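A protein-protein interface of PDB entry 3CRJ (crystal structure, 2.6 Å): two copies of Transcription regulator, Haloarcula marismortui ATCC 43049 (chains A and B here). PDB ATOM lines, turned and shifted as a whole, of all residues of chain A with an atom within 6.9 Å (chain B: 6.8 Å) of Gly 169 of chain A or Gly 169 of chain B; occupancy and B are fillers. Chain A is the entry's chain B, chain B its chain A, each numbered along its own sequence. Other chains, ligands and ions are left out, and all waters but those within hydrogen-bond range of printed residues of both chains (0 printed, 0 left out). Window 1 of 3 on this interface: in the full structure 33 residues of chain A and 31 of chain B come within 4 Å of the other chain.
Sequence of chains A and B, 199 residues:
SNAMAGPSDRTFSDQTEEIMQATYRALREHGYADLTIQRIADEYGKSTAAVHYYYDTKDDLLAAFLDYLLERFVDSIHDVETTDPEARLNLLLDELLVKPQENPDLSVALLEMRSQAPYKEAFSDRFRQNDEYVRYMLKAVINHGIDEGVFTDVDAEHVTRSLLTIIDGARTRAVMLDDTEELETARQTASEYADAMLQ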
ATOM      1  N   LEU A 164      -5.715  30.125   9.505  1.00  0.00           N
ATOM      2  CA  LEU A 164      -5.022  29.063  10.226  1.00  0.00           C
ATOM      3  C   LEU A 164      -3.698  28.670   9.564  1.00  0.00           C
ATOM      4  O   LEU A 164      -2.722  28.340  10.247  1.00  0.00           O
ATOM      5  CB  LEU A 164      -5.920  27.826  10.369  1.00  0.00           C
ATOM      6  CG  LEU A 164      -6.719  27.699  11.682  1.00  0.00           C
ATOM      7  CD1 LEU A 164      -5.807  27.803  12.890  1.00  0.00           C
ATOM      8  CD2 LEU A 164      -7.771  28.768  11.785  1.00  0.00           C
ATOM      9  N   THR A 165      -3.651  28.701   8.240  1.00  0.00           N
ATOM     10  CA  THR A 165      -2.412  28.412   7.565  1.00  0.00           C
ATOM     11  C   THR A 165      -1.408  29.489   7.974  1.00  0.00           C
ATOM     12  O   THR A 165      -0.325  29.178   8.445  1.00  0.00           O
ATOM     13  CB  THR A 165      -2.656  28.350   6.068  1.00  0.00           C
ATOM     14  OG1 THR A 165      -3.631  27.347   5.852  1.00  0.00           O
ATOM     15  CG2 THR A 165      -1.410  27.963   5.305  1.00  0.00           C
ATOM     16  N   ILE A 166      -1.796  30.752   7.853  1.00  0.00           N
ATOM     17  CA  ILE A 166      -0.936  31.850   8.284  1.00  0.00           C
ATOM     18  C   ILE A 166      -0.484  31.677   9.769  1.00  0.00           C
ATOM     19  O   ILE A 166       0.711  31.791  10.068  1.00  0.00           O
ATOM     20  CB  ILE A 166      -1.611  33.220   8.022  1.00  0.00           C
ATOM     21  CG1 ILE A 166      -1.768  33.446   6.523  1.00  0.00           C
ATOM     22  CG2 ILE A 166      -0.843  34.359   8.650  1.00  0.00           C
ATOM     23  CD1 ILE A 166      -2.887  34.421   6.177  1.00  0.00           C
ATOM     24  N   ILE A 167      -1.416  31.370  10.681  1.00  0.00           N
ATOM     25  CA  ILE A 167      -1.075  31.253  12.110  1.00  0.00           C
ATOM     26  C   ILE A 167      -0.098  30.102  12.333  1.00  0.00           C
ATOM     27  O   ILE A 167       0.928  30.276  13.003  1.00  0.00           O
ATOM     28  CB  ILE A 167      -2.337  31.117  13.007  1.00  0.00           C
ATOM     29  CG1 ILE A 167      -3.109  32.421  13.018  1.00  0.00           C
ATOM     30  CG2 ILE A 167      -1.987  30.709  14.450  1.00  0.00           C
ATOM     31  CD1 ILE A 167      -4.568  32.223  13.278  1.00  0.00           C
ATOM     32  N   ASP A 168      -0.382  28.948  11.729  1.00  0.00           N
ATOM     33  CA  ASP A 168       0.497  27.779  11.882  1.00  0.00           C
ATOM     34  C   ASP A 168       1.895  27.964  11.275  1.00  0.00           C
ATOM     35  O   ASP A 168       2.898  27.580  11.880  1.00  0.00           O
ATOM     36  CB  ASP A 168      -0.179  26.489  11.397  1.00  0.00           C
ATOM     37  CG  ASP A 168      -1.163  25.907  12.433  1.00  0.00           C
ATOM     38  OD1 ASP A 168      -0.889  25.962  13.658  1.00  0.00           O
ATOM     39  OD2 ASP A 168      -2.218  25.380  12.031  1.00  0.00           O
ATOM     40  N   GLY A 169       1.970  28.577  10.109  1.00  0.00           N
ATOM     41  CA  GLY A 169       3.272  28.904   9.517  1.00  0.00           C
ATOM     42  C   GLY A 169       4.093  29.807  10.422  1.00  0.00           C
ATOM     43  O   GLY A 169       5.297  29.589  10.592  1.00  0.00           O
ATOM     44  N   ALA A 170       3.433  30.807  11.027  1.00  0.00           N
ATOM     45  CA  ALA A 170       4.081  31.718  11.982  1.00  0.00           C
ATOM     46  C   ALA A 170       4.670  30.965  13.172  1.00  0.00           C
ATOM     47  O   ALA A 170       5.783  31.245  13.591  1.00  0.00           O
ATOM     48  CB  ALA A 170       3.123  32.776  12.465  1.00  0.00           C
ATOM     49  N   ARG A 171       3.919  30.018  13.721  1.00  0.00           N
ATOM     50  CA  ARG A 171       4.398  29.281  14.881  1.00  0.00           C
ATOM     51  C   ARG A 171       5.635  28.471  14.502  1.00  0.00           C
ATOM     52  O   ARG A 171       6.626  28.465  15.227  1.00  0.00           O
ATOM     53  CB  ARG A 171       3.296  28.379  15.468  1.00  0.00           C
ATOM     54  CG  ARG A 171       2.182  29.117  16.221  1.00  0.00           C
ATOM     55  CD  ARG A 171       0.940  28.211  16.361  1.00  0.00           C
ATOM     56  NE  ARG A 171      -0.142  28.883  17.104  1.00  0.00           N
ATOM     57  CZ  ARG A 171      -1.415  28.468  17.192  1.00  0.00           C
ATOM     58  NH1 ARG A 171      -1.848  27.356  16.582  1.00  0.00           N
ATOM     59  NH2 ARG A 171      -2.269  29.191  17.908  1.00  0.00           N
ATOM     60  N   THR A 172       5.567  27.823  13.338  1.00  0.00           N
ATOM     61  CA  THR A 172       6.661  27.005  12.801  1.00  0.00           C
ATOM     62  C   THR A 172       7.888  27.851  12.517  1.00  0.00           C
ATOM     63  O   THR A 172       9.008  27.536  12.972  1.00  0.00           O
ATOM     64  CB  THR A 172       6.235  26.320  11.497  1.00  0.00           C
ATOM     65  OG1 THR A 172       5.078  25.509  11.748  1.00  0.00           O
ATOM     66  CG2 THR A 172       7.351  25.457  10.949  1.00  0.00           C
ATOM     67  N   ARG A 173       7.680  28.927  11.764  1.00  0.00           N
ATOM     68  CA  ARG A 173       8.789  29.750  11.339  1.00  0.00           C
ATOM     69  C   ARG A 173       9.479  30.429  12.504  1.00  0.00           C
ATOM     70  O   ARG A 173      10.690  30.578  12.497  1.00  0.00           O
ATOM     71  CB  ARG A 173       8.329  30.749  10.307  1.00  0.00           C
ATOM     72  CG  ARG A 173       7.988  30.117   9.005  1.00  0.00           C
ATOM     73  CD  ARG A 173       7.559  31.169   7.998  1.00  0.00           C
ATOM     74  NE  ARG A 173       8.593  32.184   7.765  1.00  0.00           N
ATOM     75  CZ  ARG A 173       9.592  32.046   6.900  1.00  0.00           C
ATOM     76  NH1 ARG A 173       9.712  30.921   6.204  1.00  0.00           N
ATOM     77  NH2 ARG A 173      10.476  33.022   6.723  1.00  0.00           N
ATOM     78  N   ALA A 174       8.712  30.804  13.521  1.00  0.00           N
ATOM     79  CA  ALA A 174       9.271  31.476  14.684  1.00  0.00           C
ATOM     80  C   ALA A 174      10.241  30.604  15.463  1.00  0.00           C
ATOM     81  O   ALA A 174      11.216  31.117  16.000  1.00  0.00           O
ATOM     82  CB  ALA A 174       8.190  32.017  15.588  1.00  0.00           C
ATOM     83  N   VAL A 175      10.011  29.294  15.522  1.00  0.00           N
ATOM     84  CA  VAL A 175      11.038  28.448  16.141  1.00  0.00           C
ATOM     85  C   VAL A 175      12.122  28.009  15.168  1.00  0.00           C
ATOM     86  O   VAL A 175      13.314  28.001  15.535  1.00  0.00           O
ATOM     87  CB  VAL A 175      10.516  27.220  16.962  1.00  0.00           C
ATOM     88  CG1 VAL A 175       9.055  27.369  17.340  1.00  0.00           C
ATOM     89  CG2 VAL A 175      10.759  25.936  16.231  1.00  0.00           C
ATOM     90  N   GLU A 182       8.761  36.836  13.722  1.00  0.00           N
ATOM     91  CA  GLU A 182       8.127  36.027  12.723  1.00  0.00           C
ATOM     92  C   GLU A 182       6.597  35.959  12.978  1.00  0.00           C
ATOM     93  O   GLU A 182       5.785  35.868  12.043  1.00  0.00           O
ATOM     94  CB  GLU A 182       8.801  34.665  12.794  1.00  0.00           C
ATOM     95  CG  GLU A 182       8.638  33.774  11.605  1.00  0.00           C
ATOM     96  CD  GLU A 182       9.467  34.167  10.418  1.00  0.00           C
ATOM     97  OE1 GLU A 182       8.868  34.373   9.354  1.00  0.00           O
ATOM     98  OE2 GLU A 182      10.696  34.262  10.527  1.00  0.00           O
ATOM     99  N   LEU A 183       6.205  36.039  14.249  1.00  0.00           N
ATOM    100  CA  LEU A 183       4.798  36.195  14.608  1.00  0.00           C
ATOM    101  C   LEU A 183       4.266  37.611  14.332  1.00  0.00           C
ATOM    102  O   LEU A 183       3.100  37.750  14.000  1.00  0.00           O
ATOM    103  CB  LEU A 183       4.548  35.791  16.058  1.00  0.00           C
ATOM    104  CG  LEU A 183       4.953  34.370  16.493  1.00  0.00           C
ATOM    105  CD1 LEU A 183       5.306  34.320  17.983  1.00  0.00           C
ATOM    106  CD2 LEU A 183       3.885  33.324  16.145  1.00  0.00           C
ATOM    107  N   ALA A 186       3.450  37.889  10.547  1.00  0.00           N
ATOM    108  CA  ALA A 186       2.231  37.081  10.344  1.00  0.00           C
ATOM    109  C   ALA A 186       0.965  37.780  10.830  1.00  0.00           C
ATOM    110  O   ALA A 186      -0.115  37.573  10.270  1.00  0.00           O
ATOM    111  CB  ALA A 186       2.378  35.733  11.027  1.00  0.00           C
ATOM    112  N   LEU B 164       5.915  33.158   2.446  1.00  0.00           N
ATOM    113  CA  LEU B 164       6.754  32.157   3.117  1.00  0.00           C
ATOM    114  C   LEU B 164       5.985  31.533   4.256  1.00  0.00           C
ATOM    115  O   LEU B 164       6.129  30.333   4.522  1.00  0.00           O
ATOM    116  CB  LEU B 164       8.043  32.779   3.660  1.00  0.00           C
ATOM    117  CG  LEU B 164       9.362  32.613   2.903  1.00  0.00           C
ATOM    118  CD1 LEU B 164       9.158  32.314   1.409  1.00  0.00           C
ATOM    119  CD2 LEU B 164      10.240  33.871   3.112  1.00  0.00           C
ATOM    120  N   THR B 165       5.184  32.362   4.926  1.00  0.00           N
ATOM    121  CA  THR B 165       4.421  31.910   6.064  1.00  0.00           C
ATOM    122  C   THR B 165       3.338  30.942   5.620  1.00  0.00           C
ATOM    123  O   THR B 165       3.221  29.837   6.161  1.00  0.00           O
ATOM    124  CB  THR B 165       3.836  33.076   6.862  1.00  0.00           C
ATOM    125  OG1 THR B 165       4.903  33.943   7.276  1.00  0.00           O
ATOM    126  CG2 THR B 165       3.102  32.540   8.085  1.00  0.00           C
ATOM    127  N   ILE B 166       2.577  31.349   4.612  1.00  0.00           N
ATOM    128  CA  ILE B 166       1.580  30.481   3.979  1.00  0.00           C
ATOM    129  C   ILE B 166       2.250  29.151   3.649  1.00  0.00           C
ATOM    130  O   ILE B 166       1.788  28.118   4.109  1.00  0.00           O
ATOM    131  CB  ILE B 166       0.895  31.174   2.749  1.00  0.00           C
ATOM    132  CG1 ILE B 166       0.082  32.370   3.228  1.00  0.00           C
ATOM    133  CG2 ILE B 166       0.029  30.206   1.942  1.00  0.00           C
ATOM    134  CD1 ILE B 166      -0.142  33.416   2.173  1.00  0.00           C
ATOM    135  N   ILE B 167       3.367  29.169   2.922  1.00  0.00           N
ATOM    136  CA  ILE B 167       4.049  27.918   2.582  1.00  0.00           C
ATOM    137  C   ILE B 167       4.321  27.058   3.824  1.00  0.00           C
ATOM    138  O   ILE B 167       3.930  25.879   3.879  1.00  0.00           O
ATOM    139  CB  ILE B 167       5.382  28.136   1.879  1.00  0.00           C
ATOM    140  CG1 ILE B 167       5.234  29.071   0.676  1.00  0.00           C
ATOM    141  CG2 ILE B 167       6.019  26.764   1.474  1.00  0.00           C
ATOM    142  CD1 ILE B 167       4.257  28.581  -0.292  1.00  0.00           C
ATOM    143  N   ASP B 168       4.982  27.634   4.821  1.00  0.00           N
ATOM    144  CA  ASP B 168       5.287  26.859   6.010  1.00  0.00           C
ATOM    145  C   ASP B 168       4.047  26.459   6.792  1.00  0.00           C
ATOM    146  O   ASP B 168       4.073  25.437   7.463  1.00  0.00           O
ATOM    147  CB  ASP B 168       6.338  27.529   6.894  1.00  0.00           C
ATOM    148  CG  ASP B 168       7.747  27.411   6.298  1.00  0.00           C
ATOM    149  OD1 ASP B 168       8.096  26.334   5.737  1.00  0.00           O
ATOM    150  OD2 ASP B 168       8.512  28.400   6.367  1.00  0.00           O
ATOM    151  N   GLY B 169       2.974  27.246   6.699  1.00  0.00           N
ATOM    152  CA  GLY B 169       1.721  26.869   7.325  1.00  0.00           C
ATOM    153  C   GLY B 169       1.210  25.560   6.763  1.00  0.00           C
ATOM    154  O   GLY B 169       0.898  24.611   7.505  1.00  0.00           O
ATOM    155  N   ALA B 170       1.129  25.521   5.435  1.00  0.00           N
ATOM    156  CA  ALA B 170       0.642  24.370   4.704  1.00  0.00           C
ATOM    157  C   ALA B 170       1.433  23.114   5.052  1.00  0.00           C
ATOM    158  O   ALA B 170       0.840  22.066   5.273  1.00  0.00           O
ATOM    159  CB  ALA B 170       0.725  24.653   3.225  1.00  0.00           C
ATOM    160  N   ARG B 171       2.761  23.204   5.105  1.00  0.00           N
ATOM    161  CA  ARG B 171       3.573  22.007   5.328  1.00  0.00           C
ATOM    162  C   ARG B 171       3.363  21.415   6.727  1.00  0.00           C
ATOM    163  O   ARG B 171       3.458  20.197   6.908  1.00  0.00           O
ATOM    164  CB  ARG B 171       5.067  22.274   5.130  1.00  0.00           C
ATOM    165  CG  ARG B 171       5.509  22.584   3.751  1.00  0.00           C
ATOM    166  CD  ARG B 171       6.768  23.388   3.885  1.00  0.00           C
ATOM    167  NE  ARG B 171       7.460  23.601   2.625  1.00  0.00           N
ATOM    168  CZ  ARG B 171       8.527  24.388   2.499  1.00  0.00           C
ATOM    169  NH1 ARG B 171       9.014  25.029   3.551  1.00  0.00           N
ATOM    170  NH2 ARG B 171       9.107  24.550   1.323  1.00  0.00           N
ATOM    171  N   THR B 172       3.118  22.279   7.706  1.00  0.00           N
ATOM    172  CA  THR B 172       2.907  21.837   9.066  1.00  0.00           C
ATOM    173  C   THR B 172       1.533  21.199   9.193  1.00  0.00           C
ATOM    174  O   THR B 172       1.400  20.124   9.809  1.00  0.00           O
ATOM    175  CB  THR B 172       3.017  22.992  10.063  1.00  0.00           C
ATOM    176  OG1 THR B 172       4.221  23.712   9.805  1.00  0.00           O
ATOM    177  CG2 THR B 172       3.098  22.476  11.466  1.00  0.00           C
ATOM    178  N   ARG B 173       0.518  21.845   8.623  1.00  0.00           N
ATOM    179  CA  ARG B 173      -0.852  21.392   8.796  1.00  0.00           C
ATOM    180  C   ARG B 173      -1.090  20.139   7.968  1.00  0.00           C
ATOM    181  O   ARG B 173      -1.923  19.301   8.320  1.00  0.00           O
ATOM    182  CB  ARG B 173      -1.854  22.481   8.420  1.00  0.00           C
ATOM    183  CG  ARG B 173      -1.762  23.756   9.228  1.00  0.00           C
ATOM    184  CD  ARG B 173      -2.785  24.808   8.749  1.00  0.00           C
ATOM    185  NE  ARG B 173      -4.140  24.264   8.754  1.00  0.00           N
ATOM    186  CZ  ARG B 173      -4.910  24.187   9.832  1.00  0.00           C
ATOM    187  NH1 ARG B 173      -4.476  24.637  11.008  1.00  0.00           N
ATOM    188  NH2 ARG B 173      -6.121  23.655   9.744  1.00  0.00           N
ATOM    189  N   ALA B 174      -0.354  20.006   6.869  1.00  0.00           N
ATOM    190  CA  ALA B 174      -0.501  18.814   6.039  1.00  0.00           C
ATOM    191  C   ALA B 174      -0.018  17.604   6.805  1.00  0.00           C
ATOM    192  O   ALA B 174      -0.671  16.577   6.765  1.00  0.00           O
ATOM    193  CB  ALA B 174       0.218  18.938   4.697  1.00  0.00           C
ATOM    194  N   MET B 176       0.610  17.616  10.331  1.00  0.00           N
ATOM    195  CA  MET B 176      -0.111  17.628  11.627  1.00  0.00           C
ATOM    196  C   MET B 176      -1.556  17.116  11.474  1.00  0.00           C
ATOM    197  O   MET B 176      -2.103  16.521  12.395  1.00  0.00           O
ATOM    198  CB  MET B 176      -0.094  19.022  12.265  1.00  0.00           C
ATOM    199  CG  MET B 176      -0.427  19.106  13.769  1.00  0.00           C
ATOM    200  SD  MET B 176      -1.509  20.764  14.263  1.00  0.00           S
ATOM    201  CE  MET B 176      -0.937  22.011  12.875  1.00  0.00           C
ATOM    202  N   GLU B 182      -4.374  20.352   2.626  1.00  0.00           N
ATOM    203  CA  GLU B 182      -3.881  21.548   3.270  1.00  0.00           C
ATOM    204  C   GLU B 182      -2.981  22.392   2.372  1.00  0.00           C
ATOM    205  O   GLU B 182      -2.963  23.632   2.463  1.00  0.00           O
ATOM    206  CB  GLU B 182      -3.075  21.175   4.502  1.00  0.00           C
ATOM    207  CG  GLU B 182      -3.885  20.548   5.587  1.00  0.00           C
ATOM    208  CD  GLU B 182      -4.767  21.524   6.326  1.00  0.00           C
ATOM    209  OE1 GLU B 182      -5.779  21.062   6.896  1.00  0.00           O
ATOM    210  OE2 GLU B 182      -4.447  22.731   6.373  1.00  0.00           O
ATOM    211  N   LEU B 183      -2.224  21.716   1.518  1.00  0.00           N
ATOM    212  CA  LEU B 183      -1.400  22.407   0.568  1.00  0.00           C
ATOM    213  C   LEU B 183      -2.277  22.968  -0.540  1.00  0.00           C
ATOM    214  O   LEU B 183      -2.000  24.049  -1.072  1.00  0.00           O
ATOM    215  CB  LEU B 183      -0.331  21.463  -0.002  1.00  0.00           C
ATOM    216  CG  LEU B 183       0.522  20.646   0.975  1.00  0.00           C
ATOM    217  CD1 LEU B 183       1.205  19.478   0.264  1.00  0.00           C
ATOM    218  CD2 LEU B 183       1.533  21.519   1.665  1.00  0.00           C
ATOM    219  N   ALA B 186      -3.873  26.007   0.774  1.00  0.00           N
ATOM    220  CA  ALA B 186      -2.801  27.013   0.889  1.00  0.00           C
ATOM    221  C   ALA B 186      -2.364  27.584  -0.459  1.00  0.00           C
ATOM    222  O   ALA B 186      -2.048  28.766  -0.564  1.00  0.00           O
ATOM    223  CB  ALA B 186      -1.603  26.476   1.645  1.00  0.00           C
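The guanidinium group of Arg 171 of chain B lies within salt-bridge range of the side-chain carboxylate of Asp 168 of chain B, at 2.7 Å.
The backbone carbonyl oxygen (O) of Asp 168 of chain B is in hydrogen-bond range of the side-chain hydroxyl (OG1) of Thr 172 of chain B (2.9 Å).
The guanidinium group (NE) of Arg 173 of chain B lies within salt-bridge range of the side-chain carboxylate (OE2) of Glu 182 of chain B, at 2.8 Å.
The side-chain carboxylate (OD1) of Asp 168 of chain A is in salt-bridge range of the guanidinium group (NH1) of Arg 171 of chain A.
The backbone carbonyl oxygen (O) of Asp 168 of chain A lies within hydrogen-bond range of the side-chain hydroxyl (OG1) of Thr 172 of chain A (3.0 Å).
The guanidinium group (NE) of Arg 173 of chain A lies within salt-bridge range of the side-chain carboxylate (OE1) of Glu 182 of chain A (2.7 Å).
Of the 15 printed residues of chain B, 10 touch a printed residue of chain A.
Printed residues of chain B that touch a printed residue of chain A: Leu 164, Thr 165, Ile 166, Asp 168, Gly 169, Ala 170, Thr 172, Arg 173, Met 176 and Ala 186.
Hydrophobic or aromatic side chains of chain B that line the printed part of chain A: Leu 164, Ile 166, Met 176 and Ala 186.
Hydrophobic or aromatic side chains of chain A within 4 Å of the printed part of chain B: Leu 164 and Ile 166.
Among the printed residues, Asp or Glu carboxylates within 4 Å of a Lys or Arg side-chain nitrogen of the other chain: Asp 168 of chain A with Arg 173 of chain B (2.6 Å) and Arg 173 of chain A with Asp 168 of chain B (2.8 Å).
Of the printed residues of chain B, Thr 165 of chain A touches Ile 166 (3.4 Å), Gly 169 (3.3 Å), Ala 170 (3.5 Å), Arg 173 (3.8 Å) and Ala 186 (3.96 Å).
Gly 169 of chain A touches just these residues of chain B: Thr 165 (3.5 Å), Asp 168 (3.7 Å) and Gly 169 (3.3 Å).
Val 175 of chain A touches none of the printed residues of chain B.
Of the printed residues of chain A, Thr 165 of chain B touches Ile 166 (3.2 Å), Gly 169 (3.5 Å), Ala 170 (3.4 Å) and Arg 173 (3.8 Å).
Of the printed residues of chain A, Ile 166 of chain B touches Thr 165 and Ile 166.
Of chain A, only Thr 165 and Gly 169 come within 4 Å of Gly 169 of chain B.
The nearest residue of chain B that does not touch Gly 169 of chain A is Thr 172 of chain B (5.3 Å).
The side-chain carboxylate of Asp 168 of chain B lies within salt-bridge range of the guanidinium group of Arg 173 of chain A, at 2.8 Å.
The side-chain hydroxyl (OG1) of Thr 172 of chain B lies within hydrogen-bond range of the side-chain hydroxyl (OG1) of Thr 172 of chain A (2.8 Å).
The side-chain carboxylate (OD2) of Asp 168 of chain A lies within salt-bridge range of the guanidinium group (NH1) of Arg 173 of chain B (2.6 Å).
Among the printed residues, merely in contact across the chains: Leu 164 of chain A with Arg 173 of chain B (3.6 Å), Thr 165 of chain A with Ile 166 of chain B (3.4 Å), Thr 165 of chain A with Gly 169 of chain B (3.3 Å), Thr 165 of chain A with Ala 170 of chain B (3.5 Å), Thr 165 of chain A with Arg 173 of chain B (3.8 Å), Thr 165 of chain A with Ala 186 of chain B (3.96 Å), Ile 166 of chain A with Thr 165 of chain B (3.2 Å), Ile 166 of chain A with Ile 166 of chain B (3.9 Å), Asp 168 of chain A with Met 176 of chain B (3.7 Å), Gly 169 of chain A with Thr 165 of chain B (3.5 Å), Gly 169 of chain A with Asp 168 of chain B (3.7 Å), Gly 169 of chain A with Gly 169 of chain B (3.3 Å), Ala 170 of chain A with Thr 165 of chain B (3.4 Å), Arg 173 of chain A with Leu 164 of chain B (3.6 Å) and Arg 173 of chain A with Thr 165 of chain B (3.8 Å).
Leu 164 of chain A touches Arg 173 of chain B, and with the chains exchanged Arg 173 of chain A touches Leu 164 of chain B.
Thr 165 of chain A touches Ala 186 of chain B, but with the chains exchanged Ala 186 of chain A does not touch Thr 165 of chain B (4.4 Å).
Gly 169 of chain A touches Asp 168 of chain B, but with the chains exchanged Asp 168 of chain A does not touch Gly 169 of chain B (4.1 Å).
Thr 172 of chain B touches its own counterpart, Thr 172 of chain A.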
